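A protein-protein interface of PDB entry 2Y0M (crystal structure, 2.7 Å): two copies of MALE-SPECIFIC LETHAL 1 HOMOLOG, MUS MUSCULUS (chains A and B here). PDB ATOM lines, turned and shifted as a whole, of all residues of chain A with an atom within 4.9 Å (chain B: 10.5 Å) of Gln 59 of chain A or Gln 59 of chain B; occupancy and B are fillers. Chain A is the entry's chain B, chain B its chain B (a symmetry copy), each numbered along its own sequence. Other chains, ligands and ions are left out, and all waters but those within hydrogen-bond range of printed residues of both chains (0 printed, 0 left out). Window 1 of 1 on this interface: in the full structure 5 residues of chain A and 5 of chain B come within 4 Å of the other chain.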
ATOM      1  N   ARG A  55     -17.055  12.609   2.594  1.00  0.00           N
ATOM      2  CA  ARG A  55     -16.699  14.024   2.757  1.00  0.00           C
ATOM      3  C   ARG A  55     -17.783  14.912   2.165  1.00  0.00           C
ATOM      4  O   ARG A  55     -18.109  15.960   2.724  1.00  0.00           O
ATOM      5  CB  ARG A  55     -15.368  14.356   2.074  1.00  0.00           C
ATOM      6  CG  ARG A  55     -14.160  13.575   2.546  1.00  0.00           C
ATOM      7  CD  ARG A  55     -12.953  13.939   1.689  1.00  0.00           C
ATOM      8  NE  ARG A  55     -12.233  12.756   1.219  1.00  0.00           N
ATOM      9  CZ  ARG A  55     -11.102  12.300   1.745  1.00  0.00           C
ATOM     10  NH1 ARG A  55     -10.534  12.928   2.770  1.00  0.00           N
ATOM     11  NH2 ARG A  55     -10.532  11.212   1.242  1.00  0.00           N
ATOM     12  N   TRP A  56     -18.320  14.485   1.024  1.00  0.00           N
ATOM     13  CA  TRP A  56     -19.407  15.184   0.346  1.00  0.00           C
ATOM     14  C   TRP A  56     -20.640  15.302   1.245  1.00  0.00           C
ATOM     15  O   TRP A  56     -21.197  16.392   1.402  1.00  0.00           O
ATOM     16  CB  TRP A  56     -19.764  14.473  -0.964  1.00  0.00           C
ATOM     17  CG  TRP A  56     -20.750  15.226  -1.811  1.00  0.00           C
ATOM     18  CD1 TRP A  56     -22.111  15.234  -1.678  1.00  0.00           C
ATOM     19  CD2 TRP A  56     -20.452  16.081  -2.922  1.00  0.00           C
ATOM     20  NE1 TRP A  56     -22.676  16.044  -2.633  1.00  0.00           N
ATOM     21  CE2 TRP A  56     -21.682  16.574  -3.411  1.00  0.00           C
ATOM     22  CE3 TRP A  56     -19.265  16.478  -3.552  1.00  0.00           C
ATOM     23  CZ2 TRP A  56     -21.760  17.444  -4.501  1.00  0.00           C
ATOM     24  CZ3 TRP A  56     -19.344  17.345  -4.637  1.00  0.00           C
ATOM     25  CH2 TRP A  56     -20.584  17.816  -5.099  1.00  0.00           C
ATOM     26  N   ASP A  57     -21.051  14.181   1.837  1.00  0.00           N
ATOM     27  CA  ASP A  57     -22.249  14.139   2.670  1.00  0.00           C
ATOM     28  C   ASP A  57     -22.095  14.920   3.970  1.00  0.00           C
ATOM     29  O   ASP A  57     -23.045  15.564   4.418  1.00  0.00           O
ATOM     30  CB  ASP A  57     -22.669  12.691   2.957  1.00  0.00           C
ATOM     31  CG  ASP A  57     -23.395  12.045   1.785  1.00  0.00           C
ATOM     32  OD1 ASP A  57     -23.841  12.770   0.868  1.00  0.00           O
ATOM     33  OD2 ASP A  57     -23.525  10.800   1.789  1.00  0.00           O
ATOM     34  N   ILE A  58     -20.905  14.858   4.569  1.00  0.00           N
ATOM     35  CA  ILE A  58     -20.620  15.621   5.788  1.00  0.00           C
ATOM     36  C   ILE A  58     -20.789  17.117   5.523  1.00  0.00           C
ATOM     37  O   ILE A  58     -21.426  17.824   6.305  1.00  0.00           O
ATOM     38  CB  ILE A  58     -19.216  15.301   6.369  1.00  0.00           C
ATOM     39  CG1 ILE A  58     -19.227  13.917   7.035  1.00  0.00           C
ATOM     40  CG2 ILE A  58     -18.780  16.370   7.378  1.00  0.00           C
ATOM     41  CD1 ILE A  58     -17.847  13.307   7.265  1.00  0.00           C
ATOM     42  N   GLN A  59     -20.240  17.583   4.404  1.00  0.00           N
ATOM     43  CA  GLN A  59     -20.358  18.981   4.016  1.00  0.00           C
ATOM     44  C   GLN A  59     -21.804  19.341   3.663  1.00  0.00           C
ATOM     45  O   GLN A  59     -22.290  20.406   4.045  1.00  0.00           O
ATOM     46  CB  GLN A  59     -19.418  19.292   2.850  1.00  0.00           C
ATOM     47  CG  GLN A  59     -19.317  20.769   2.506  1.00  0.00           C
ATOM     48  CD  GLN A  59     -18.156  21.089   1.585  1.00  0.00           C
ATOM     49  OE1 GLN A  59     -17.174  20.346   1.510  1.00  0.00           O
ATOM     50  NE2 GLN A  59     -18.259  22.212   0.882  1.00  0.00           N
ATOM     51  N   ARG A  60     -22.479  18.446   2.946  1.00  0.00           N
ATOM     52  CA  ARG A  60     -23.859  18.663   2.515  1.00  0.00           C
ATOM     53  C   ARG A  60     -24.818  18.802   3.704  1.00  0.00           C
ATOM     54  O   ARG A  60     -25.683  19.681   3.708  1.00  0.00           O
ATOM     55  CB  ARG A  60     -24.307  17.538   1.570  1.00  0.00           C
ATOM     56  CG  ARG A  60     -25.669  17.742   0.912  1.00  0.00           C
ATOM     57  CD  ARG A  60     -25.595  18.549  -0.389  1.00  0.00           C
ATOM     58  NE  ARG A  60     -25.264  19.967  -0.196  1.00  0.00           N
ATOM     59  CZ  ARG A  60     -26.112  20.899   0.251  1.00  0.00           C
ATOM     60  NH1 ARG A  60     -27.368  20.586   0.572  1.00  0.00           N
ATOM     61  NH2 ARG A  60     -25.698  22.155   0.378  1.00  0.00           N
ATOM     62  N   ILE A  61     -24.645  17.942   4.707  1.00  0.00           N
ATOM     63  CA  ILE A  61     -25.446  17.972   5.933  1.00  0.00           C
ATOM     64  C   ILE A  61     -25.163  19.234   6.758  1.00  0.00           C
ATOM     65  O   ILE A  61     -26.093  19.869   7.265  1.00  0.00           O
ATOM     66  CB  ILE A  61     -25.245  16.677   6.776  1.00  0.00           C
ATOM     67  CG1 ILE A  61     -25.980  15.501   6.120  1.00  0.00           C
ATOM     68  CG2 ILE A  61     -25.726  16.864   8.220  1.00  0.00           C
ATOM     69  CD1 ILE A  61     -25.459  14.128   6.516  1.00  0.00           C
ATOM     70  N   ARG A  62     -23.886  19.595   6.874  1.00  0.00           N
ATOM     71  CA  ARG A  62     -23.484  20.810   7.588  1.00  0.00           C
ATOM     72  C   ARG A  62     -24.038  22.074   6.940  1.00  0.00           C
ATOM     73  O   ARG A  62     -24.439  23.005   7.635  1.00  0.00           O
ATOM     74  CB  ARG A  62     -21.961  20.908   7.707  1.00  0.00           C
ATOM     75  CG  ARG A  62     -21.401  20.296   8.982  1.00  0.00           C
ATOM     76  CD  ARG A  62     -19.990  20.790   9.274  1.00  0.00           C
ATOM     77  NE  ARG A  62     -19.951  22.226   9.554  1.00  0.00           N
ATOM     78  CZ  ARG A  62     -18.851  22.907   9.868  1.00  0.00           C
ATOM     79  NH1 ARG A  62     -17.676  22.290   9.951  1.00  0.00           N
ATOM     80  NH2 ARG A  62     -18.926  24.210  10.104  1.00  0.00           N
ATOM     81  N   GLU A  63     -24.059  22.095   5.610  1.00  0.00           N
ATOM     82  CA  GLU A  63     -24.595  23.225   4.858  1.00  0.00           C
ATOM     83  C   GLU A  63     -26.108  23.342   5.015  1.00  0.00           C
ATOM     84  O   GLU A  63     -26.639  24.445   5.170  1.00  0.00           O
ATOM     85  CB  GLU A  63     -24.215  23.117   3.381  1.00  0.00           C
ATOM     86  CG  GLU A  63     -22.768  23.500   3.085  1.00  0.00           C
ATOM     87  CD  GLU A  63     -22.360  23.211   1.652  1.00  0.00           C
ATOM     88  OE1 GLU A  63     -22.986  22.339   1.014  1.00  0.00           O
ATOM     89  OE2 GLU A  63     -21.405  23.850   1.169  1.00  0.00           O
ATOM     90  N   LYS B  51      -5.849  22.030   3.030  1.00  0.00           N
ATOM     91  CA  LYS B  51      -6.375  20.943   2.208  1.00  0.00           C
ATOM     92  C   LYS B  51      -7.878  20.763   2.411  1.00  0.00           C
ATOM     93  O   LYS B  51      -8.614  20.573   1.442  1.00  0.00           O
ATOM     94  CB  LYS B  51      -5.622  19.636   2.473  1.00  0.00           C
ATOM     95  CG  LYS B  51      -4.382  19.459   1.611  1.00  0.00           C
ATOM     96  CD  LYS B  51      -3.559  18.251   2.036  1.00  0.00           C
ATOM     97  CE  LYS B  51      -2.379  18.041   1.099  1.00  0.00           C
ATOM     98  NZ  LYS B  51      -1.367  17.107   1.664  1.00  0.00           N
ATOM     99  N   ARG B  52      -8.322  20.848   3.667  1.00  0.00           N
ATOM    100  CA  ARG B  52      -9.743  20.735   4.010  1.00  0.00           C
ATOM    101  C   ARG B  52     -10.559  21.906   3.467  1.00  0.00           C
ATOM    102  O   ARG B  52     -11.667  21.712   2.968  1.00  0.00           O
ATOM    103  CB  ARG B  52      -9.934  20.610   5.527  1.00  0.00           C
ATOM    104  CG  ARG B  52      -9.438  19.299   6.109  1.00  0.00           C
ATOM    105  CD  ARG B  52      -9.540  19.280   7.625  1.00  0.00           C
ATOM    106  NE  ARG B  52      -8.518  18.416   8.215  1.00  0.00           N
ATOM    107  CZ  ARG B  52      -8.511  17.998   9.480  1.00  0.00           C
ATOM    108  NH1 ARG B  52      -9.482  18.353  10.316  1.00  0.00           N
ATOM    109  NH2 ARG B  52      -7.530  17.215   9.910  1.00  0.00           N
ATOM    110  N   ARG B  53     -10.002  23.114   3.561  1.00  0.00           N
ATOM    111  CA  ARG B  53     -10.643  24.317   3.021  1.00  0.00           C
ATOM    112  C   ARG B  53     -10.733  24.289   1.497  1.00  0.00           C
ATOM    113  O   ARG B  53     -11.660  24.856   0.913  1.00  0.00           O
ATOM    114  CB  ARG B  53      -9.906  25.575   3.477  1.00  0.00           C
ATOM    115  CG  ARG B  53     -10.288  26.048   4.866  1.00  0.00           C
ATOM    116  CD  ARG B  53      -9.277  27.048   5.391  1.00  0.00           C
ATOM    117  NE  ARG B  53      -9.713  27.674   6.637  1.00  0.00           N
ATOM    118  CZ  ARG B  53      -8.901  28.292   7.492  1.00  0.00           C
ATOM    119  NH1 ARG B  53      -7.595  28.362   7.252  1.00  0.00           N
ATOM    120  NH2 ARG B  53      -9.396  28.834   8.598  1.00  0.00           N
ATOM    121  N   LYS B  54      -9.767  23.628   0.865  1.00  0.00           N
ATOM    122  CA  LYS B  54      -9.740  23.495  -0.587  1.00  0.00           C
ATOM    123  C   LYS B  54     -10.806  22.508  -1.064  1.00  0.00           C
ATOM    124  O   LYS B  54     -11.418  22.720  -2.109  1.00  0.00           O
ATOM    125  CB  LYS B  54      -8.341  23.086  -1.074  1.00  0.00           C
ATOM    126  CG  LYS B  54      -8.070  23.412  -2.535  1.00  0.00           C
ATOM    127  CD  LYS B  54      -6.612  23.170  -2.916  1.00  0.00           C
ATOM    128  CE  LYS B  54      -6.327  23.659  -4.338  1.00  0.00           C
ATOM    129  NZ  LYS B  54      -4.903  23.453  -4.755  1.00  0.00           N
ATOM    130  N   ARG B  55     -11.023  21.442  -0.292  1.00  0.00           N
ATOM    131  CA  ARG B  55     -12.087  20.470  -0.576  1.00  0.00           C
ATOM    132  C   ARG B  55     -13.452  21.118  -0.404  1.00  0.00           C
ATOM    133  O   ARG B  55     -14.374  20.852  -1.177  1.00  0.00           O
ATOM    134  CB  ARG B  55     -12.003  19.253   0.349  1.00  0.00           C
ATOM    135  CG  ARG B  55     -10.711  18.465   0.306  1.00  0.00           C
ATOM    136  CD  ARG B  55     -10.748  17.368   1.364  1.00  0.00           C
ATOM    137  NE  ARG B  55      -9.526  17.333   2.166  1.00  0.00           N
ATOM    138  CZ  ARG B  55      -8.537  16.461   2.003  1.00  0.00           C
ATOM    139  NH1 ARG B  55      -8.614  15.525   1.062  1.00  0.00           N
ATOM    140  NH2 ARG B  55      -7.468  16.522   2.787  1.00  0.00           N
ATOM    141  N   TRP B  56     -13.569  21.955   0.625  1.00  0.00           N
ATOM    142  CA  TRP B  56     -14.790  22.702   0.908  1.00  0.00           C
ATOM    143  C   TRP B  56     -15.178  23.601  -0.269  1.00  0.00           C
ATOM    144  O   TRP B  56     -16.327  23.581  -0.719  1.00  0.00           O
ATOM    145  CB  TRP B  56     -14.624  23.533   2.185  1.00  0.00           C
ATOM    146  CG  TRP B  56     -15.892  24.194   2.646  1.00  0.00           C
ATOM    147  CD1 TRP B  56     -16.419  25.370   2.189  1.00  0.00           C
ATOM    148  CD2 TRP B  56     -16.792  23.716   3.654  1.00  0.00           C
ATOM    149  NE1 TRP B  56     -17.593  25.650   2.846  1.00  0.00           N
ATOM    150  CE2 TRP B  56     -17.845  24.653   3.751  1.00  0.00           C
ATOM    151  CE3 TRP B  56     -16.812  22.588   4.484  1.00  0.00           C
ATOM    152  CZ2 TRP B  56     -18.906  24.497   4.647  1.00  0.00           C
ATOM    153  CZ3 TRP B  56     -17.870  22.433   5.374  1.00  0.00           C
ATOM    154  CH2 TRP B  56     -18.900  23.385   5.447  1.00  0.00           C
ATOM    155  N   ASP B  57     -14.215  24.375  -0.766  1.00  0.00           N
ATOM    156  CA  ASP B  57     -14.463  25.325  -1.847  1.00  0.00           C
ATOM    157  C   ASP B  57     -14.775  24.643  -3.174  1.00  0.00           C
ATOM    158  O   ASP B  57     -15.621  25.125  -3.930  1.00  0.00           O
ATOM    159  CB  ASP B  57     -13.289  26.299  -2.005  1.00  0.00           C
ATOM    160  CG  ASP B  57     -13.296  27.405  -0.958  1.00  0.00           C
ATOM    161  OD1 ASP B  57     -14.337  27.613  -0.296  1.00  0.00           O
ATOM    162  OD2 ASP B  57     -12.250  28.076  -0.805  1.00  0.00           O
ATOM    163  N   ILE B  58     -14.094  23.531  -3.453  1.00  0.00           N
ATOM    164  CA  ILE B  58     -14.356  22.755  -4.668  1.00  0.00           C
ATOM    165  C   ILE B  58     -15.808  22.274  -4.680  1.00  0.00           C
ATOM    166  O   ILE B  58     -16.502  22.402  -5.690  1.00  0.00           O
ATOM    167  CB  ILE B  58     -13.364  21.573  -4.838  1.00  0.00           C
ATOM    168  CG1 ILE B  58     -11.988  22.101  -5.270  1.00  0.00           C
ATOM    169  CG2 ILE B  58     -13.886  20.557  -5.862  1.00  0.00           C
ATOM    170  CD1 ILE B  58     -10.834  21.123  -5.066  1.00  0.00           C
ATOM    171  N   GLN B  59     -16.265  21.751  -3.545  1.00  0.00           N
ATOM    172  CA  GLN B  59     -17.639  21.288  -3.413  1.00  0.00           C
ATOM    173  C   GLN B  59     -18.628  22.454  -3.478  1.00  0.00           C
ATOM    174  O   GLN B  59     -19.673  22.349  -4.122  1.00  0.00           O
ATOM    175  CB  GLN B  59     -17.813  20.496  -2.116  1.00  0.00           C
ATOM    176  CG  GLN B  59     -19.156  19.799  -1.985  1.00  0.00           C
ATOM    177  CD  GLN B  59     -19.188  18.771  -0.870  1.00  0.00           C
ATOM    178  OE1 GLN B  59     -18.153  18.249  -0.450  1.00  0.00           O
ATOM    179  NE2 GLN B  59     -20.390  18.466  -0.392  1.00  0.00           N
ATOM    180  N   ARG B  60     -18.286  23.559  -2.818  1.00  0.00           N
ATOM    181  CA  ARG B  60     -19.142  24.743  -2.770  1.00  0.00           C
ATOM    182  C   ARG B  60     -19.367  25.346  -4.162  1.00  0.00           C
ATOM    183  O   ARG B  60     -20.493  25.715  -4.506  1.00  0.00           O
ATOM    184  CB  ARG B  60     -18.560  25.784  -1.802  1.00  0.00           C
ATOM    185  CG  ARG B  60     -19.451  26.993  -1.530  1.00  0.00           C
ATOM    186  CD  ARG B  60     -20.447  26.763  -0.387  1.00  0.00           C
ATOM    187  NE  ARG B  60     -21.515  25.808  -0.706  1.00  0.00           N
ATOM    188  CZ  ARG B  60     -22.573  26.070  -1.480  1.00  0.00           C
ATOM    189  NH1 ARG B  60     -22.730  27.269  -2.043  1.00  0.00           N
ATOM    190  NH2 ARG B  60     -23.481  25.124  -1.692  1.00  0.00           N
ATOM    191  N   ILE B  61     -18.298  25.427  -4.951  1.00  0.00           N
ATOM    192  CA  ILE B  61     -18.355  25.935  -6.325  1.00  0.00           C
ATOM    193  C   ILE B  61     -19.152  24.997  -7.238  1.00  0.00           C
ATOM    194  O   ILE B  61     -19.968  25.455  -8.045  1.00  0.00           O
ATOM    195  CB  ILE B  61     -16.928  26.210  -6.889  1.00  0.00           C
ATOM    196  CG1 ILE B  61     -16.347  27.483  -6.259  1.00  0.00           C
ATOM    197  CG2 ILE B  61     -16.940  26.332  -8.417  1.00  0.00           C
ATOM    198  CD1 ILE B  61     -14.830  27.578  -6.306  1.00  0.00           C
ATOM    199  N   ARG B  62     -18.924  23.691  -7.096  1.00  0.00           N
ATOM    200  CA  ARG B  62     -19.660  22.685  -7.867  1.00  0.00           C
ATOM    201  C   ARG B  62     -21.155  22.706  -7.571  1.00  0.00           C
ATOM    202  O   ARG B  62     -21.971  22.538  -8.474  1.00  0.00           O
ATOM    203  CB  ARG B  62     -19.099  21.281  -7.629  1.00  0.00           C
ATOM    204  CG  ARG B  62     -18.025  20.869  -8.624  1.00  0.00           C
ATOM    205  CD  ARG B  62     -17.817  19.360  -8.639  1.00  0.00           C
ATOM    206  NE  ARG B  62     -19.000  18.641  -9.115  1.00  0.00           N
ATOM    207  CZ  ARG B  62     -19.077  17.319  -9.254  1.00  0.00           C
ATOM    208  NH1 ARG B  62     -18.036  16.547  -8.956  1.00  0.00           N
ATOM    209  NH2 ARG B  62     -20.200  16.766  -9.695  1.00  0.00           N
ATOM    210  N   GLU B  63     -21.503  22.916  -6.304  1.00  0.00           N
ATOM    211  CA  GLU B  63     -22.897  22.996  -5.883  1.00  0.00           C
ATOM    212  C   GLU B  63     -23.578  24.254  -6.415  1.00  0.00           C
ATOM    213  O   GLU B  63     -24.728  24.206  -6.858  1.00  0.00           O
ATOM    214  CB  GLU B  63     -23.004  22.933  -4.359  1.00  0.00           C
ATOM    215  CG  GLU B  63     -22.825  21.531  -3.784  1.00  0.00           C
ATOM    216  CD  GLU B  63     -22.750  21.517  -2.268  1.00  0.00           C
ATOM    217  OE1 GLU B  63     -22.389  22.556  -1.676  1.00  0.00           O
ATOM    218  OE2 GLU B  63     -23.042  20.462  -1.671  1.00  0.00           O
ATOM    219  N   GLN B  64     -22.855  25.373  -6.380  1.00  0.00           N
ATOM    220  CA  GLN B  64     -23.351  26.641  -6.910  1.00  0.00           C
ATOM    221  C   GLN B  64     -23.628  26.561  -8.405  1.00  0.00           C
ATOM    222  O   GLN B  64     -24.649  27.068  -8.878  1.00  0.00           O
ATOM    223  CB  GLN B  64     -22.369  27.771  -6.617  1.00  0.00           C
ATOM    224  CG  GLN B  64     -22.492  28.337  -5.217  1.00  0.00           C
ATOM    225  CD  GLN B  64     -21.412  29.349  -4.891  1.00  0.00           C
ATOM    226  OE1 GLN B  64     -21.068  30.204  -5.712  1.00  0.00           O
ATOM    227  NE2 GLN B  64     -20.877  29.265  -3.679  1.00  0.00           N
ATOM    228  N   ARG B  65     -22.724  25.909  -9.134  1.00  0.00           N
ATOM    229  CA  ARG B  65     -22.843  25.753 -10.585  1.00  0.00           C
ATOM    230  C   ARG B  65     -24.041  24.897 -10.996  1.00  0.00           C
ATOM    231  O   ARG B  65     -24.688  25.175 -12.010  1.00  0.00           O
ATOM    232  CB  ARG B  65     -21.547  25.187 -11.175  1.00  0.00           C
ATOM    233  CG  ARG B  65     -20.470  26.238 -11.395  1.00  0.00           C
ATOM    234  CD  ARG B  65     -19.154  25.614 -11.819  1.00  0.00           C
ATOM    235  NE  ARG B  65     -18.130  26.628 -12.063  1.00  0.00           N
ATOM    236  CZ  ARG B  65     -16.819  26.395 -12.075  1.00  0.00           C
ATOM    237  NH1 ARG B  65     -16.350  25.174 -11.846  1.00  0.00           N
ATOM    238  NH2 ARG B  65     -15.972  27.389 -12.308  1.00  0.00           N
ATOM    239  N   ILE B  66     -24.334  23.869 -10.203  1.00  0.00           N
ATOM    240  CA  ILE B  66     -25.478  22.991 -10.452  1.00  0.00           C
ATOM    241  C   ILE B  66     -26.811  23.714 -10.206  1.00  0.00           C
ATOM    242  O   ILE B  66     -27.739  23.605 -11.014  1.00  0.00           O
ATOM    243  CB  ILE B  66     -25.385  21.682  -9.616  1.00  0.00           C
ATOM    244  CG1 ILE B  66     -24.224  20.814 -10.113  1.00  0.00           C
ATOM    245  CG2 ILE B  66     -26.691  20.893  -9.677  1.00  0.00           C
ATOM    246  CD1 ILE B  66     -23.704  19.808  -9.094  1.00  0.00           C
ATOM    247  N   LEU B  67     -26.887  24.462  -9.107  1.00  0.00           N
ATOM    248  CA  LEU B  67     -28.129  25.125  -8.695  1.00  0.00           C
ATOM    249  C   LEU B  67     -28.576  26.267  -9.610  1.00  0.00           C
ATOM    250  O   LEU B  67     -29.772  26.429  -9.859  1.00  0.00           O
ATOM    251  CB  LEU B  67     -28.037  25.613  -7.242  1.00  0.00           C
ATOM    252  CG  LEU B  67     -28.017  24.562  -6.126  1.00  0.00           C
ATOM    253  CD1 LEU B  67     -27.722  25.207  -4.782  1.00  0.00           C
ATOM    254  CD2 LEU B  67     -29.318  23.771  -6.064  1.00  0.00           C
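Arg 55 of chain A touches Gln 59 of chain B, and with the chains exchanged Gln 59 of chain A touches Arg 55 of chain B. Trp 56 of chain A touches Gln 59 of chain B, and with the chains exchanged Gln 59 of chain A touches Trp 56 of chain B. Gln 59 of chain A touches its own counterpart, Gln 59 of chain B. Arg 60 of chain A touches Glu 63 of chain B, and with the chains exchanged Glu 63 of chain A touches Arg 60 of chain B. Of the 11 pairs that touch across the chains among the printed residues, 11 have their exchanged pair printed and touching as well.
Printed residues of chain B within 4 Å of Arg 55 of chain A: Arg 55 (3.7 Å) and Gln 59 (3.9 Å). No residue of chain B comes within 4 Å of Ile 58 of chain A. Of chain B, only Arg 55 (3.9 Å), Trp 56 (2.9 Å), Gln 59 (3.0 Å) and Arg 60 (3.9 Å) come within 4 Å of Gln 59 of chain A. Ile 61 of chain A touches none of the printed residues of chain B. Of the printed residues of chain B, Glu 63 of chain A touches Arg 60 and Glu 63. Printed residues of chain A within 4 Å of Arg 55 of chain B: Arg 55 and Gln 59. Of the printed residues of chain A, Trp 56 of chain B touches Gln 59 (2.9 Å). Of the printed residues of chain A, Arg 60 of chain B touches Gln 59 (3.9 Å) and Glu 63 (2.7 Å). Of the printed residues of chain A, Glu 63 of chain B touches Arg 60 (2.7 Å) and Glu 63 (2.8 Å). The nearest printed residue of chain B that does not touch Gln 59 of chain A is Glu 63 of chain B (4.9 Å). The nearest printed residue of chain B that does not touch Arg 55 of chain A is Trp 56 of chain B (7.0 Å).
Of the 17 printed residues of chain B, 5 touch a printed residue of chain A. Printed residues of chain B that touch a printed residue of chain A: Arg 55, Trp 56, Gln 59, Arg 60 and Glu 63. Hydrophobic or aromatic side chains of chain B within 4 Å of the printed part of chain A: Trp 56. Among the printed residues, Asp or Glu carboxylates within 4 Å of a Lys or Arg side-chain nitrogen of the other chain: Arg 60 of chain A with Glu 63 of chain B and Glu 63 of chain A with Arg 60 of chain B.
Among the printed residues, pairs that only touch across the chains: Arg 55 of chain A with Arg 55 of chain B (3.7 Å), Arg 55 of chain A with Gln 59 of chain B (3.9 Å), Gln 59 of chain A with Arg 55 of chain B (3.9 Å), Gln 59 of chain A with Arg 60 of chain B (3.9 Å) and Arg 60 of chain A with Gln 59 of chain B (3.9 Å).
The backbone carbonyl oxygen of Trp 56 of chain A lies within hydrogen-bond range of the side-chain amide nitrogen of Gln 59 of chain B, 2.9 Å away. NE2 of Gln 59 of chain A is in hydrogen-bond range of O of Trp 56 of chain B. The side-chain amide oxygen (OE1) of Gln 59 of chain A sits close to the side-chain amide oxygen (OE1) of Gln 59 of chain B. OE2 of Glu 63 of chain B is in salt-bridge range of NE of Arg 60 of chain A, 2.7 Å away. The guanidinium group of Arg 60 of chain B lies within salt-bridge range of the side-chain carboxylate of Glu 63 of chain A (2.7 Å). OE1 of Glu 63 of chain B lies close to OE1 of Glu 63 of chain A (2.8 Å).
NH2 of Arg 60 of chain A is in salt-bridge range of OE1 of Glu 63 of chain A (2.8 Å). The backbone carbonyl oxygen of Lys 51 of chain B lies close to the guanidinium group of Arg 55 of chain B (3.4 Å). The guanidinium group (NH2) of Arg 60 of chain B lies within salt-bridge range of the side-chain carboxylate (OE1) of Glu 63 of chain B (2.8 Å). NH1 of Arg 60 of chain B sits close to NE2 of Gln 64 of chain B (3.2 Å).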
